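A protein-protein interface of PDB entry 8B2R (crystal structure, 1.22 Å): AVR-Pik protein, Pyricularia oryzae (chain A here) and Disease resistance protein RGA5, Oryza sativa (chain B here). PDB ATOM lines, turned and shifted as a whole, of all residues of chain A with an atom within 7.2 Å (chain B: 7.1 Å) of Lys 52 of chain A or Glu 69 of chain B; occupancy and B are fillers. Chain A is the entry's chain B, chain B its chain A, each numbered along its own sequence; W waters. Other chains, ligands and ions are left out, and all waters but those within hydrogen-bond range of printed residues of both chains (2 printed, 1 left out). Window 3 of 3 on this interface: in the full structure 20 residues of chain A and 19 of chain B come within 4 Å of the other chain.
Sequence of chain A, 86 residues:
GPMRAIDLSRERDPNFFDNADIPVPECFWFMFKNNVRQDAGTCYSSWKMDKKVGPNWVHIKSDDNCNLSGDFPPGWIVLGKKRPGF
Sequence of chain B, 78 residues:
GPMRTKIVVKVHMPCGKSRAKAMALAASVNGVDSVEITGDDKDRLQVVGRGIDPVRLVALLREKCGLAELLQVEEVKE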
ATOM      1  N   TRP A  29     -12.551 -37.975   6.543  1.00  0.00           N
ATOM      2  CA  TRP A  29     -11.671 -36.857   6.352  1.00  0.00           C
ATOM      3  C   TRP A  29     -11.945 -35.828   7.437  1.00  0.00           C
ATOM      4  O   TRP A  29     -13.066 -35.691   7.959  1.00  0.00           O
ATOM      5  CB  TRP A  29     -11.759 -36.231   4.932  1.00  0.00           C
ATOM      6  CG  TRP A  29     -13.106 -35.694   4.587  1.00  0.00           C
ATOM      7  CD1 TRP A  29     -14.028 -36.350   3.816  1.00  0.00           C
ATOM      8  CD2 TRP A  29     -13.700 -34.450   4.986  1.00  0.00           C
ATOM      9  NE1 TRP A  29     -15.139 -35.593   3.744  1.00  0.00           N
ATOM     10  CE2 TRP A  29     -14.987 -34.424   4.425  1.00  0.00           C
ATOM     11  CE3 TRP A  29     -13.227 -33.343   5.723  1.00  0.00           C
ATOM     12  CZ2 TRP A  29     -15.877 -33.376   4.642  1.00  0.00           C
ATOM     13  CZ3 TRP A  29     -14.112 -32.297   5.896  1.00  0.00           C
ATOM     14  CH2 TRP A  29     -15.421 -32.315   5.379  1.00  0.00           C
ATOM     15  N   MET A  31     -10.785 -31.640   8.386  1.00  0.00           N
ATOM     16  CA  MET A  31     -10.224 -30.415   7.856  1.00  0.00           C
ATOM     17  C   MET A  31      -9.893 -29.482   9.010  1.00  0.00           C
ATOM     18  O   MET A  31     -10.697 -29.281   9.932  1.00  0.00           O
ATOM     19  CB  MET A  31     -11.272 -29.724   6.990  1.00  0.00           C
ATOM     20  CG  MET A  31     -10.709 -28.473   6.303  1.00  0.00           C
ATOM     21  SD  MET A  31     -11.631 -27.909   4.894  1.00  0.00           S
ATOM     22  CE  MET A  31     -13.035 -27.362   5.770  1.00  0.00           C
ATOM     23  N   ASP A  39     -14.230 -28.953  10.051  1.00  0.00           N
ATOM     24  CA  ASP A  39     -15.276 -29.789   9.496  1.00  0.00           C
ATOM     25  C   ASP A  39     -14.705 -31.209   9.413  1.00  0.00           C
ATOM     26  O   ASP A  39     -13.483 -31.416   9.501  1.00  0.00           O
ATOM     27  CB  ASP A  39     -15.846 -29.239   8.185  1.00  0.00           C
ATOM     28  CG  ASP A  39     -17.221 -29.785   7.770  1.00  0.00           C
ATOM     29  OD1 ASP A  39     -17.870 -30.535   8.574  1.00  0.00           O
ATOM     30  OD2 ASP A  39     -17.654 -29.354   6.697  1.00  0.00           O
ATOM     31  N   ASP A  50     -13.923 -33.248  -4.929  1.00  0.00           N
ATOM     32  CA  ASP A  50     -13.714 -31.810  -4.960  1.00  0.00           C
ATOM     33  C   ASP A  50     -14.290 -31.246  -3.671  1.00  0.00           C
ATOM     34  O   ASP A  50     -15.394 -31.619  -3.280  1.00  0.00           O
ATOM     35  CB  ASP A  50     -14.328 -31.238  -6.220  1.00  0.00           C
ATOM     36  CG  ASP A  50     -13.634 -31.838  -7.444  1.00  0.00           C
ATOM     37  OD1 ASP A  50     -12.434 -31.616  -7.593  1.00  0.00           O
ATOM     38  OD2 ASP A  50     -14.315 -32.533  -8.293  1.00  0.00           O
ATOM     39  N   LYS A  51     -13.517 -30.393  -3.013  1.00  0.00           N
ATOM     40  CA  LYS A  51     -13.796 -29.978  -1.649  1.00  0.00           C
ATOM     41  C   LYS A  51     -13.511 -28.507  -1.446  1.00  0.00           C
ATOM     42  O   LYS A  51     -12.469 -28.010  -1.844  1.00  0.00           O
ATOM     43  CB  LYS A  51     -12.894 -30.835  -0.759  1.00  0.00           C
ATOM     44  CG  LYS A  51     -13.066 -30.671   0.720  1.00  0.00           C
ATOM     45  CD  LYS A  51     -14.274 -31.316   1.291  1.00  0.00           C
ATOM     46  CE  LYS A  51     -14.792 -30.702   2.573  1.00  0.00           C
ATOM     47  NZ  LYS A  51     -15.311 -29.304   2.442  1.00  0.00           N
ATOM     48  N   LYS A  52     -14.411 -27.846  -0.702  1.00  0.00           N
ATOM     49  CA  LYS A  52     -14.157 -26.486  -0.256  1.00  0.00           C
ATOM     50  C   LYS A  52     -13.221 -26.523   0.943  1.00  0.00           C
ATOM     51  O   LYS A  52     -13.485 -27.203   1.928  1.00  0.00           O
ATOM     52  CB  LYS A  52     -15.455 -25.776   0.107  1.00  0.00           C
ATOM     53  CG  LYS A  52     -15.343 -24.280   0.390  1.00  0.00           C
ATOM     54  CD  LYS A  52     -15.008 -23.477  -0.881  1.00  0.00           C
ATOM     55  CE  LYS A  52     -15.197 -21.989  -0.791  1.00  0.00           C
ATOM     56  NZ  LYS A  52     -16.616 -21.616  -0.611  1.00  0.00           N
ATOM     57  N   VAL A  53     -12.086 -25.828   0.859  1.00  0.00           N
ATOM     58  CA  VAL A  53     -11.078 -25.784   1.917  1.00  0.00           C
ATOM     59  C   VAL A  53     -10.749 -24.308   2.148  1.00  0.00           C
ATOM     60  O   VAL A  53     -10.136 -23.684   1.325  1.00  0.00           O
ATOM     61  CB  VAL A  53      -9.802 -26.559   1.526  1.00  0.00           C
ATOM     62  CG1 VAL A  53      -8.799 -26.546   2.670  1.00  0.00           C
ATOM     63  CG2 VAL A  53     -10.141 -27.985   1.049  1.00  0.00           C
ATOM     64  N   GLY A  54     -11.307 -23.728   3.203  1.00  0.00           N
ATOM     65  CA  GLY A  54     -11.281 -22.294   3.423  1.00  0.00           C
ATOM     66  C   GLY A  54     -11.856 -21.561   2.216  1.00  0.00           C
ATOM     67  O   GLY A  54     -12.949 -21.884   1.768  1.00  0.00           O
ATOM     68  N   PRO A  55     -11.124 -20.613   1.592  1.00  0.00           N
ATOM     69  CA  PRO A  55     -11.625 -19.899   0.421  1.00  0.00           C
ATOM     70  C   PRO A  55     -11.446 -20.623  -0.912  1.00  0.00           C
ATOM     71  O   PRO A  55     -11.820 -20.079  -1.962  1.00  0.00           O
ATOM     72  CB  PRO A  55     -10.787 -18.615   0.401  1.00  0.00           C
ATOM     73  CG  PRO A  55      -9.491 -19.050   0.978  1.00  0.00           C
ATOM     74  CD  PRO A  55      -9.805 -20.133   1.990  1.00  0.00           C
ATOM     75  N   ASN A  56     -10.873 -21.837  -0.887  1.00  0.00           N
ATOM     76  CA  ASN A  56     -10.480 -22.485  -2.129  1.00  0.00           C
ATOM     77  C   ASN A  56     -11.294 -23.745  -2.411  1.00  0.00           C
ATOM     78  O   ASN A  56     -11.753 -24.428  -1.509  1.00  0.00           O
ATOM     79  CB  ASN A  56      -9.009 -22.872  -2.099  1.00  0.00           C
ATOM     80  CG  ASN A  56      -8.119 -21.670  -2.287  1.00  0.00           C
ATOM     81  OD1 ASN A  56      -7.849 -21.286  -3.420  1.00  0.00           O
ATOM     82  ND2 ASN A  56      -7.779 -21.006  -1.197  1.00  0.00           N
ATOM     83  N   TRP A  57     -11.410 -24.053  -3.705  1.00  0.00           N
ATOM     84  CA  TRP A  57     -12.078 -25.263  -4.191  1.00  0.00           C
ATOM     85  C   TRP A  57     -10.985 -26.195  -4.701  1.00  0.00           C
ATOM     86  O   TRP A  57     -10.265 -25.828  -5.591  1.00  0.00           O
ATOM     87  CB  TRP A  57     -13.088 -24.906  -5.286  1.00  0.00           C
ATOM     88  CG  TRP A  57     -13.906 -26.056  -5.772  1.00  0.00           C
ATOM     89  CD1 TRP A  57     -13.818 -26.675  -6.989  1.00  0.00           C
ATOM     90  CD2 TRP A  57     -14.951 -26.738  -5.064  1.00  0.00           C
ATOM     91  NE1 TRP A  57     -14.742 -27.688  -7.061  1.00  0.00           N
ATOM     92  CE2 TRP A  57     -15.454 -27.749  -5.894  1.00  0.00           C
ATOM     93  CE3 TRP A  57     -15.539 -26.570  -3.808  1.00  0.00           C
ATOM     94  CZ2 TRP A  57     -16.477 -28.623  -5.504  1.00  0.00           C
ATOM     95  CZ3 TRP A  57     -16.500 -27.446  -3.397  1.00  0.00           C
ATOM     96  CH2 TRP A  57     -16.971 -28.444  -4.242  1.00  0.00           C
ATOM     97  N   VAL A  58     -10.825 -27.333  -4.056  1.00  0.00           N
ATOM     98  CA  VAL A  58      -9.655 -28.166  -4.209  1.00  0.00           C
ATOM     99  C   VAL A  58     -10.036 -29.575  -4.645  1.00  0.00           C
ATOM    100  O   VAL A  58     -10.846 -30.241  -4.010  1.00  0.00           O
ATOM    101  CB  VAL A  58      -8.874 -28.236  -2.883  1.00  0.00           C
ATOM    102  CG1 VAL A  58      -7.623 -29.060  -3.023  1.00  0.00           C
ATOM    103  CG2 VAL A  58      -8.590 -26.845  -2.340  1.00  0.00           C
ATOM    104  N   ILE A  60      -9.087 -33.285  -4.438  1.00  0.00           N
ATOM    105  CA  ILE A  60      -8.363 -34.096  -3.480  1.00  0.00           C
ATOM    106  C   ILE A  60      -8.438 -35.567  -3.877  1.00  0.00           C
ATOM    107  O   ILE A  60      -9.510 -36.087  -4.085  1.00  0.00           O
ATOM    108  CB  ILE A  60      -8.942 -33.918  -2.076  1.00  0.00           C
ATOM    109  CG1 ILE A  60      -8.969 -32.460  -1.618  1.00  0.00           C
ATOM    110  CG2 ILE A  60      -8.264 -34.873  -1.082  1.00  0.00           C
ATOM    111  CD1 ILE A  60      -9.576 -32.271  -0.274  1.00  0.00           C
ATOM    112  N   TRP A  76      -4.285 -24.424   6.169  1.00  0.00           N
ATOM    113  CA  TRP A  76      -5.339 -25.418   6.026  1.00  0.00           C
ATOM    114  C   TRP A  76      -4.760 -26.777   5.646  1.00  0.00           C
ATOM    115  O   TRP A  76      -3.851 -26.866   4.827  1.00  0.00           O
ATOM    116  CB  TRP A  76      -6.362 -24.983   4.946  1.00  0.00           C
ATOM    117  CG  TRP A  76      -7.206 -23.792   5.294  1.00  0.00           C
ATOM    118  CD1 TRP A  76      -6.895 -22.464   5.159  1.00  0.00           C
ATOM    119  CD2 TRP A  76      -8.525 -23.807   5.867  1.00  0.00           C
ATOM    120  NE1 TRP A  76      -7.913 -21.665   5.608  1.00  0.00           N
ATOM    121  CE2 TRP A  76      -8.935 -22.461   6.034  1.00  0.00           C
ATOM    122  CE3 TRP A  76      -9.388 -24.823   6.253  1.00  0.00           C
ATOM    123  CZ2 TRP A  76     -10.167 -22.115   6.579  1.00  0.00           C
ATOM    124  CZ3 TRP A  76     -10.615 -24.494   6.777  1.00  0.00           C
ATOM    125  CH2 TRP A  76     -11.001 -23.169   6.920  1.00  0.00           C
ATOM    126  N   VAL A  78      -6.449 -31.036   4.816  1.00  0.00           N
ATOM    127  CA  VAL A  78      -7.436 -32.099   4.917  1.00  0.00           C
ATOM    128  C   VAL A  78      -6.670 -33.419   5.001  1.00  0.00           C
ATOM    129  O   VAL A  78      -5.840 -33.701   4.114  1.00  0.00           O
ATOM    130  CB  VAL A  78      -8.431 -32.106   3.748  1.00  0.00           C
ATOM    131  CG1 VAL A  78      -9.517 -33.132   3.960  1.00  0.00           C
ATOM    132  CG2 VAL A  78      -9.079 -30.752   3.592  1.00  0.00           C
ATOM    133  N   VAL B   8     -22.557 -32.203  -1.207  1.00  0.00           N
ATOM    134  CA  VAL B   8     -22.844 -31.678   0.106  1.00  0.00           C
ATOM    135  C   VAL B   8     -22.829 -30.161  -0.029  1.00  0.00           C
ATOM    136  O   VAL B   8     -21.828 -29.591  -0.471  1.00  0.00           O
ATOM    137  CB  VAL B   8     -21.841 -32.134   1.154  1.00  0.00           C
ATOM    138  CG1 VAL B   8     -22.232 -31.538   2.502  1.00  0.00           C
ATOM    139  CG2 VAL B   8     -21.709 -33.668   1.156  1.00  0.00           C
ATOM    140  N   VAL B   9     -23.937 -29.541   0.391  1.00  0.00           N
ATOM    141  CA  VAL B   9     -24.115 -28.107   0.331  1.00  0.00           C
ATOM    142  C   VAL B   9     -24.414 -27.596   1.728  1.00  0.00           C
ATOM    143  O   VAL B   9     -25.319 -28.108   2.374  1.00  0.00           O
ATOM    144  CB  VAL B   9     -25.227 -27.693  -0.625  1.00  0.00           C
ATOM    145  CG1 VAL B   9     -25.283 -26.195  -0.814  1.00  0.00           C
ATOM    146  CG2 VAL B   9     -25.144 -28.375  -1.953  1.00  0.00           C
ATOM    147  N   LYS B  10     -23.701 -26.558   2.204  1.00  0.00           N
ATOM    148  CA  LYS B  10     -24.097 -25.864   3.401  1.00  0.00           C
ATOM    149  C   LYS B  10     -25.174 -24.867   3.018  1.00  0.00           C
ATOM    150  O   LYS B  10     -24.985 -24.051   2.137  1.00  0.00           O
ATOM    151  CB  LYS B  10     -22.879 -25.138   4.001  1.00  0.00           C
ATOM    152  CG  LYS B  10     -23.138 -24.353   5.276  1.00  0.00           C
ATOM    153  CD  LYS B  10     -21.861 -23.789   5.869  1.00  0.00           C
ATOM    154  CE  LYS B  10     -22.061 -23.084   7.178  1.00  0.00           C
ATOM    155  NZ  LYS B  10     -20.783 -22.553   7.720  1.00  0.00           N
ATOM    156  N   VAL B  11     -26.282 -24.868   3.767  1.00  0.00           N
ATOM    157  CA  VAL B  11     -27.431 -24.026   3.432  1.00  0.00           C
ATOM    158  C   VAL B  11     -27.871 -23.267   4.693  1.00  0.00           C
ATOM    159  O   VAL B  11     -27.861 -23.832   5.785  1.00  0.00           O
ATOM    160  CB  VAL B  11     -28.597 -24.871   2.887  1.00  0.00           C
ATOM    161  CG1 VAL B  11     -29.798 -24.023   2.489  1.00  0.00           C
ATOM    162  CG2 VAL B  11     -28.211 -25.747   1.710  1.00  0.00           C
ATOM    163  N   HIS B  12     -28.276 -22.020   4.508  1.00  0.00           N
ATOM    164  CA  HIS B  12     -28.872 -21.293   5.595  1.00  0.00           C
ATOM    165  C   HIS B  12     -30.279 -21.830   5.846  1.00  0.00           C
ATOM    166  O   HIS B  12     -31.174 -21.668   5.002  1.00  0.00           O
ATOM    167  CB  HIS B  12     -28.968 -19.828   5.222  1.00  0.00           C
ATOM    168  CG  HIS B  12     -29.666 -19.040   6.269  1.00  0.00           C
ATOM    169  ND1 HIS B  12     -29.017 -18.810   7.468  1.00  0.00           N
ATOM    170  CD2 HIS B  12     -30.884 -18.492   6.385  1.00  0.00           C
ATOM    171  CE1 HIS B  12     -29.786 -18.109   8.273  1.00  0.00           C
ATOM    172  NE2 HIS B  12     -30.925 -17.923   7.652  1.00  0.00           N
ATOM    173  N   ARG B  44     -26.237 -28.888   6.640  1.00  0.00           N
ATOM    174  CA  ARG B  44     -25.775 -29.442   5.366  1.00  0.00           C
ATOM    175  C   ARG B  44     -26.895 -30.257   4.718  1.00  0.00           C
ATOM    176  O   ARG B  44     -27.594 -31.027   5.404  1.00  0.00           O
ATOM    177  CB  ARG B  44     -24.569 -30.365   5.530  1.00  0.00           C
ATOM    178  CG  ARG B  44     -23.203 -29.682   5.609  1.00  0.00           C
ATOM    179  CD  ARG B  44     -22.891 -29.093   6.919  1.00  0.00           C
ATOM    180  NE  ARG B  44     -21.491 -28.717   6.984  1.00  0.00           N
ATOM    181  CZ  ARG B  44     -21.017 -27.649   7.563  1.00  0.00           C
ATOM    182  NH1 ARG B  44     -21.832 -26.736   8.070  1.00  0.00           N
ATOM    183  NH2 ARG B  44     -19.705 -27.500   7.543  1.00  0.00           N
ATOM    184  N   VAL B  58     -26.771 -25.188  -6.237  1.00  0.00           N
ATOM    185  CA  VAL B  58     -26.430 -24.156  -5.276  1.00  0.00           C
ATOM    186  C   VAL B  58     -27.127 -22.837  -5.645  1.00  0.00           C
ATOM    187  O   VAL B  58     -27.641 -22.142  -4.773  1.00  0.00           O
ATOM    188  CB  VAL B  58     -24.912 -24.009  -5.096  1.00  0.00           C
ATOM    189  CG1 VAL B  58     -24.572 -22.895  -4.161  1.00  0.00           C
ATOM    190  CG2 VAL B  58     -24.318 -25.273  -4.526  1.00  0.00           C
ATOM    191  N   LEU B  61     -30.748 -23.051  -4.593  1.00  0.00           N
ATOM    192  CA  LEU B  61     -30.829 -22.966  -3.134  1.00  0.00           C
ATOM    193  C   LEU B  61     -30.564 -21.553  -2.626  1.00  0.00           C
ATOM    194  O   LEU B  61     -31.272 -21.093  -1.728  1.00  0.00           O
ATOM    195  CB  LEU B  61     -29.844 -23.941  -2.462  1.00  0.00           C
ATOM    196  CG  LEU B  61     -30.269 -25.393  -2.563  1.00  0.00           C
ATOM    197  CD1 LEU B  61     -29.132 -26.357  -2.263  1.00  0.00           C
ATOM    198  CD2 LEU B  61     -31.429 -25.683  -1.626  1.00  0.00           C
ATOM    199  N   ARG B  62     -29.593 -20.839  -3.192  1.00  0.00           N
ATOM    200  CA  ARG B  62     -29.190 -19.524  -2.731  1.00  0.00           C
ATOM    201  C   ARG B  62     -30.367 -18.570  -2.974  1.00  0.00           C
ATOM    202  O   ARG B  62     -30.680 -17.692  -2.154  1.00  0.00           O
ATOM    203  CB  ARG B  62     -27.836 -19.256  -3.416  1.00  0.00           C
ATOM    204  CG  ARG B  62     -27.159 -17.934  -3.093  1.00  0.00           C
ATOM    205  CD  ARG B  62     -25.939 -17.895  -4.004  1.00  0.00           C
ATOM    206  NE  ARG B  62     -24.947 -18.900  -3.631  1.00  0.00           N
ATOM    207  CZ  ARG B  62     -23.908 -19.280  -4.358  1.00  0.00           C
ATOM    208  NH1 ARG B  62     -23.937 -19.292  -5.684  1.00  0.00           N
ATOM    209  NH2 ARG B  62     -22.897 -19.798  -3.710  1.00  0.00           N
ATOM    210  N   LEU B  67     -28.542 -18.270   1.598  1.00  0.00           N
ATOM    211  CA  LEU B  67     -27.151 -18.598   1.482  1.00  0.00           C
ATOM    212  C   LEU B  67     -26.979 -20.081   1.288  1.00  0.00           C
ATOM    213  O   LEU B  67     -27.585 -20.888   1.965  1.00  0.00           O
ATOM    214  CB  LEU B  67     -26.468 -18.103   2.751  1.00  0.00           C
ATOM    215  CG  LEU B  67     -26.512 -16.579   2.981  1.00  0.00           C
ATOM    216  CD1 LEU B  67     -26.009 -16.197   4.374  1.00  0.00           C
ATOM    217  CD2 LEU B  67     -25.729 -15.777   1.908  1.00  0.00           C
ATOM    218  N   ALA B  68     -26.073 -20.391   0.380  1.00  0.00           N
ATOM    219  CA  ALA B  68     -25.740 -21.767   0.048  1.00  0.00           C
ATOM    220  C   ALA B  68     -24.295 -21.815  -0.434  1.00  0.00           C
ATOM    221  O   ALA B  68     -23.888 -20.965  -1.226  1.00  0.00           O
ATOM    222  CB  ALA B  68     -26.686 -22.368  -0.967  1.00  0.00           C
ATOM    223  N   GLU B  69     -23.529 -22.808   0.050  1.00  0.00           N
ATOM    224  CA  GLU B  69     -22.104 -22.962  -0.265  1.00  0.00           C
ATOM    225  C   GLU B  69     -21.841 -24.437  -0.586  1.00  0.00           C
ATOM    226  O   GLU B  69     -22.062 -25.318   0.253  1.00  0.00           O
ATOM    227  CB  GLU B  69     -21.260 -22.511   0.945  1.00  0.00           C
ATOM    228  CG  GLU B  69     -19.751 -22.618   0.773  1.00  0.00           C
ATOM    229  CD  GLU B  69     -18.981 -22.302   2.050  1.00  0.00           C
ATOM    230  OE1 GLU B  69     -19.574 -22.217   3.168  1.00  0.00           O
ATOM    231  OE2 GLU B  69     -17.758 -22.103   1.911  1.00  0.00           O
ATOM    232  N   LEU B  70     -21.312 -24.695  -1.767  1.00  0.00           N
ATOM    233  CA  LEU B  70     -20.884 -26.055  -2.076  1.00  0.00           C
ATOM    234  C   LEU B  70     -19.698 -26.447  -1.177  1.00  0.00           C
ATOM    235  O   LEU B  70     -18.713 -25.702  -1.107  1.00  0.00           O
ATOM    236  CB  LEU B  70     -20.399 -26.000  -3.518  1.00  0.00           C
ATOM    237  CG  LEU B  70     -20.320 -27.266  -4.326  1.00  0.00           C
ATOM    238  CD1 LEU B  70     -21.618 -28.063  -4.351  1.00  0.00           C
ATOM    239  CD2 LEU B  70     -19.901 -26.864  -5.725  1.00  0.00           C
ATOM    240  N   LEU B  71     -19.788 -27.604  -0.515  1.00  0.00           N
ATOM    241  CA  LEU B  71     -18.720 -28.105   0.326  1.00  0.00           C
ATOM    242  C   LEU B  71     -17.976 -29.284  -0.282  1.00  0.00           C
ATOM    243  O   LEU B  71     -16.764 -29.420  -0.013  1.00  0.00           O
ATOM    244  CB  LEU B  71     -19.236 -28.443   1.732  1.00  0.00           C
ATOM    245  CG  LEU B  71     -19.833 -27.286   2.528  1.00  0.00           C
ATOM    246  CD1 LEU B  71     -20.126 -27.767   3.943  1.00  0.00           C
ATOM    247  CD2 LEU B  71     -18.867 -26.090   2.589  1.00  0.00           C
ATOM    248  N   GLN B  72     -18.698 -30.214  -0.914  1.00  0.00           N
ATOM    249  CA  GLN B  72     -18.092 -31.452  -1.428  1.00  0.00           C
ATOM    250  C   GLN B  72     -18.867 -31.931  -2.641  1.00  0.00           C
ATOM    251  O   GLN B  72     -20.120 -31.921  -2.614  1.00  0.00           O
ATOM    252  CB  GLN B  72     -18.110 -32.507  -0.319  1.00  0.00           C
ATOM    253  CG  GLN B  72     -17.405 -33.823  -0.662  1.00  0.00           C
ATOM    254  CD  GLN B  72     -17.425 -34.776   0.531  1.00  0.00           C
ATOM    255  OE1 GLN B  72     -17.569 -34.357   1.676  1.00  0.00           O
ATOM    256  NE2 GLN B  72     -17.240 -36.071   0.262  1.00  0.00           N
ATOM    257  N   VAL B  73     -18.148 -32.295  -3.690  1.00  0.00           N
ATOM    258  CA  VAL B  73     -18.712 -33.006  -4.818  1.00  0.00           C
ATOM    259  C   VAL B  73     -17.864 -34.252  -5.006  1.00  0.00           C
ATOM    260  O   VAL B  73     -16.659 -34.161  -5.168  1.00  0.00           O
ATOM    261  CB  VAL B  73     -18.774 -32.155  -6.105  1.00  0.00           C
ATOM    262  CG1 VAL B  73     -19.374 -32.977  -7.252  1.00  0.00           C
ATOM    263  CG2 VAL B  73     -19.562 -30.887  -5.909  1.00  0.00           C
HETATM  264  O   HOH W   1     -18.076 -23.319  -2.246  1.00  0.00           O
HETATM  265  O   HOH W   2     -20.361 -31.370   8.583  1.00  0.00           O
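The guanidinium group (NH2) of Arg 44 of chain B is in salt-bridge range of the side-chain carboxylate (OD2) of Asp 39 of chain A, 2.9 Å away. The backbone NH (N) of Lys 52 of chain A lies within hydrogen-bond range of the backbone carbonyl oxygen (O) of Leu 71 of chain B (2.9 Å). The indole nitrogen (NE1) of Trp 29 of chain A is in hydrogen-bond range of the side-chain amide oxygen (OE1) of Gln 72 of chain B (3.4 Å). The backbone carbonyl oxygen of Asp 50 of chain A sits at hydrogen-bond distance from the backbone NH of Val 73 of chain B (2.9 Å). OE2 of Glu 69 of chain B is in salt-bridge range of NZ of Lys 52 of chain A. NZ of Lys 51 of chain A is in hydrogen-bond range of O of Leu 71 of chain B (2.9 Å).
N of Met 31 of chain A is in hydrogen-bond range of O of Asp 39 of chain A, at 2.9 Å. The backbone NH of Val 8 of chain B is in hydrogen-bond range of the backbone carbonyl oxygen of Gln 72 of chain B. N of Val 58 of chain A is in hydrogen-bond range of O of Lys 51 of chain A, at 2.8 Å. O of Val 8 of chain B sits at hydrogen-bond distance from N of Leu 71 of chain B, at 2.8 Å. O of Lys 10 of chain B is in hydrogen-bond range of N of Glu 69 of chain B (2.8 Å).
Among the printed residues, pairs that only touch across the chains: Asp 50 of chain A with Gln 72 of chain B (3.3 Å), Lys 52 of chain A with Leu 70 of chain B (3.5 Å), Trp 57 of chain A with Leu 70 of chain B (3.6 Å), Trp 57 of chain A with Val 73 of chain B (3.8 Å) and Trp 57 of chain A with Leu 71 of chain B (3.9 Å).
Lys 52 of chain A touches three residues of chain B. Of chain A, only Lys 52 (2.8 Å) comes within 4 Å of Glu 69 of chain B. Printed residues of chain B within 4 Å of Trp 57 of chain A: Leu 70, Leu 71 and Val 73. Printed residues of chain B within 4 Å of Trp 29 of chain A: Gln 72 (3.4 Å). Of the printed residues of chain A, Arg 44 of chain B touches Asp 39. The nearest residue of chain B that does not touch Lys 52 of chain A is Gln 72 of chain B (4.9 Å). The nearest residue of chain A that does not touch Glu 69 of chain B is Gly 54 of chain A (4.8 Å). The nearest printed residue of chain A that does not touch Val 73 of chain B is Lys 51 of chain A (5.1 Å).
Of the 16 printed residues of chain B, 6 touch a printed residue of chain A. Hydrophobic or aromatic side chains of chain B that line the printed part of chain A: Leu 70 and Val 73. Of the 15 printed residues of chain A, 6 touch a printed residue of chain B. Among the printed residues, 11 pairs touch across the chains.
Water W2 lies within hydrogen-bond range of OD1 of Asp 39 of chain A (2.6 Å) and NE of Arg 44 of chain B (3.3 Å). Water W1 bridges O of Leu 70 of chain B and NZ of Lys 52 of chain A.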
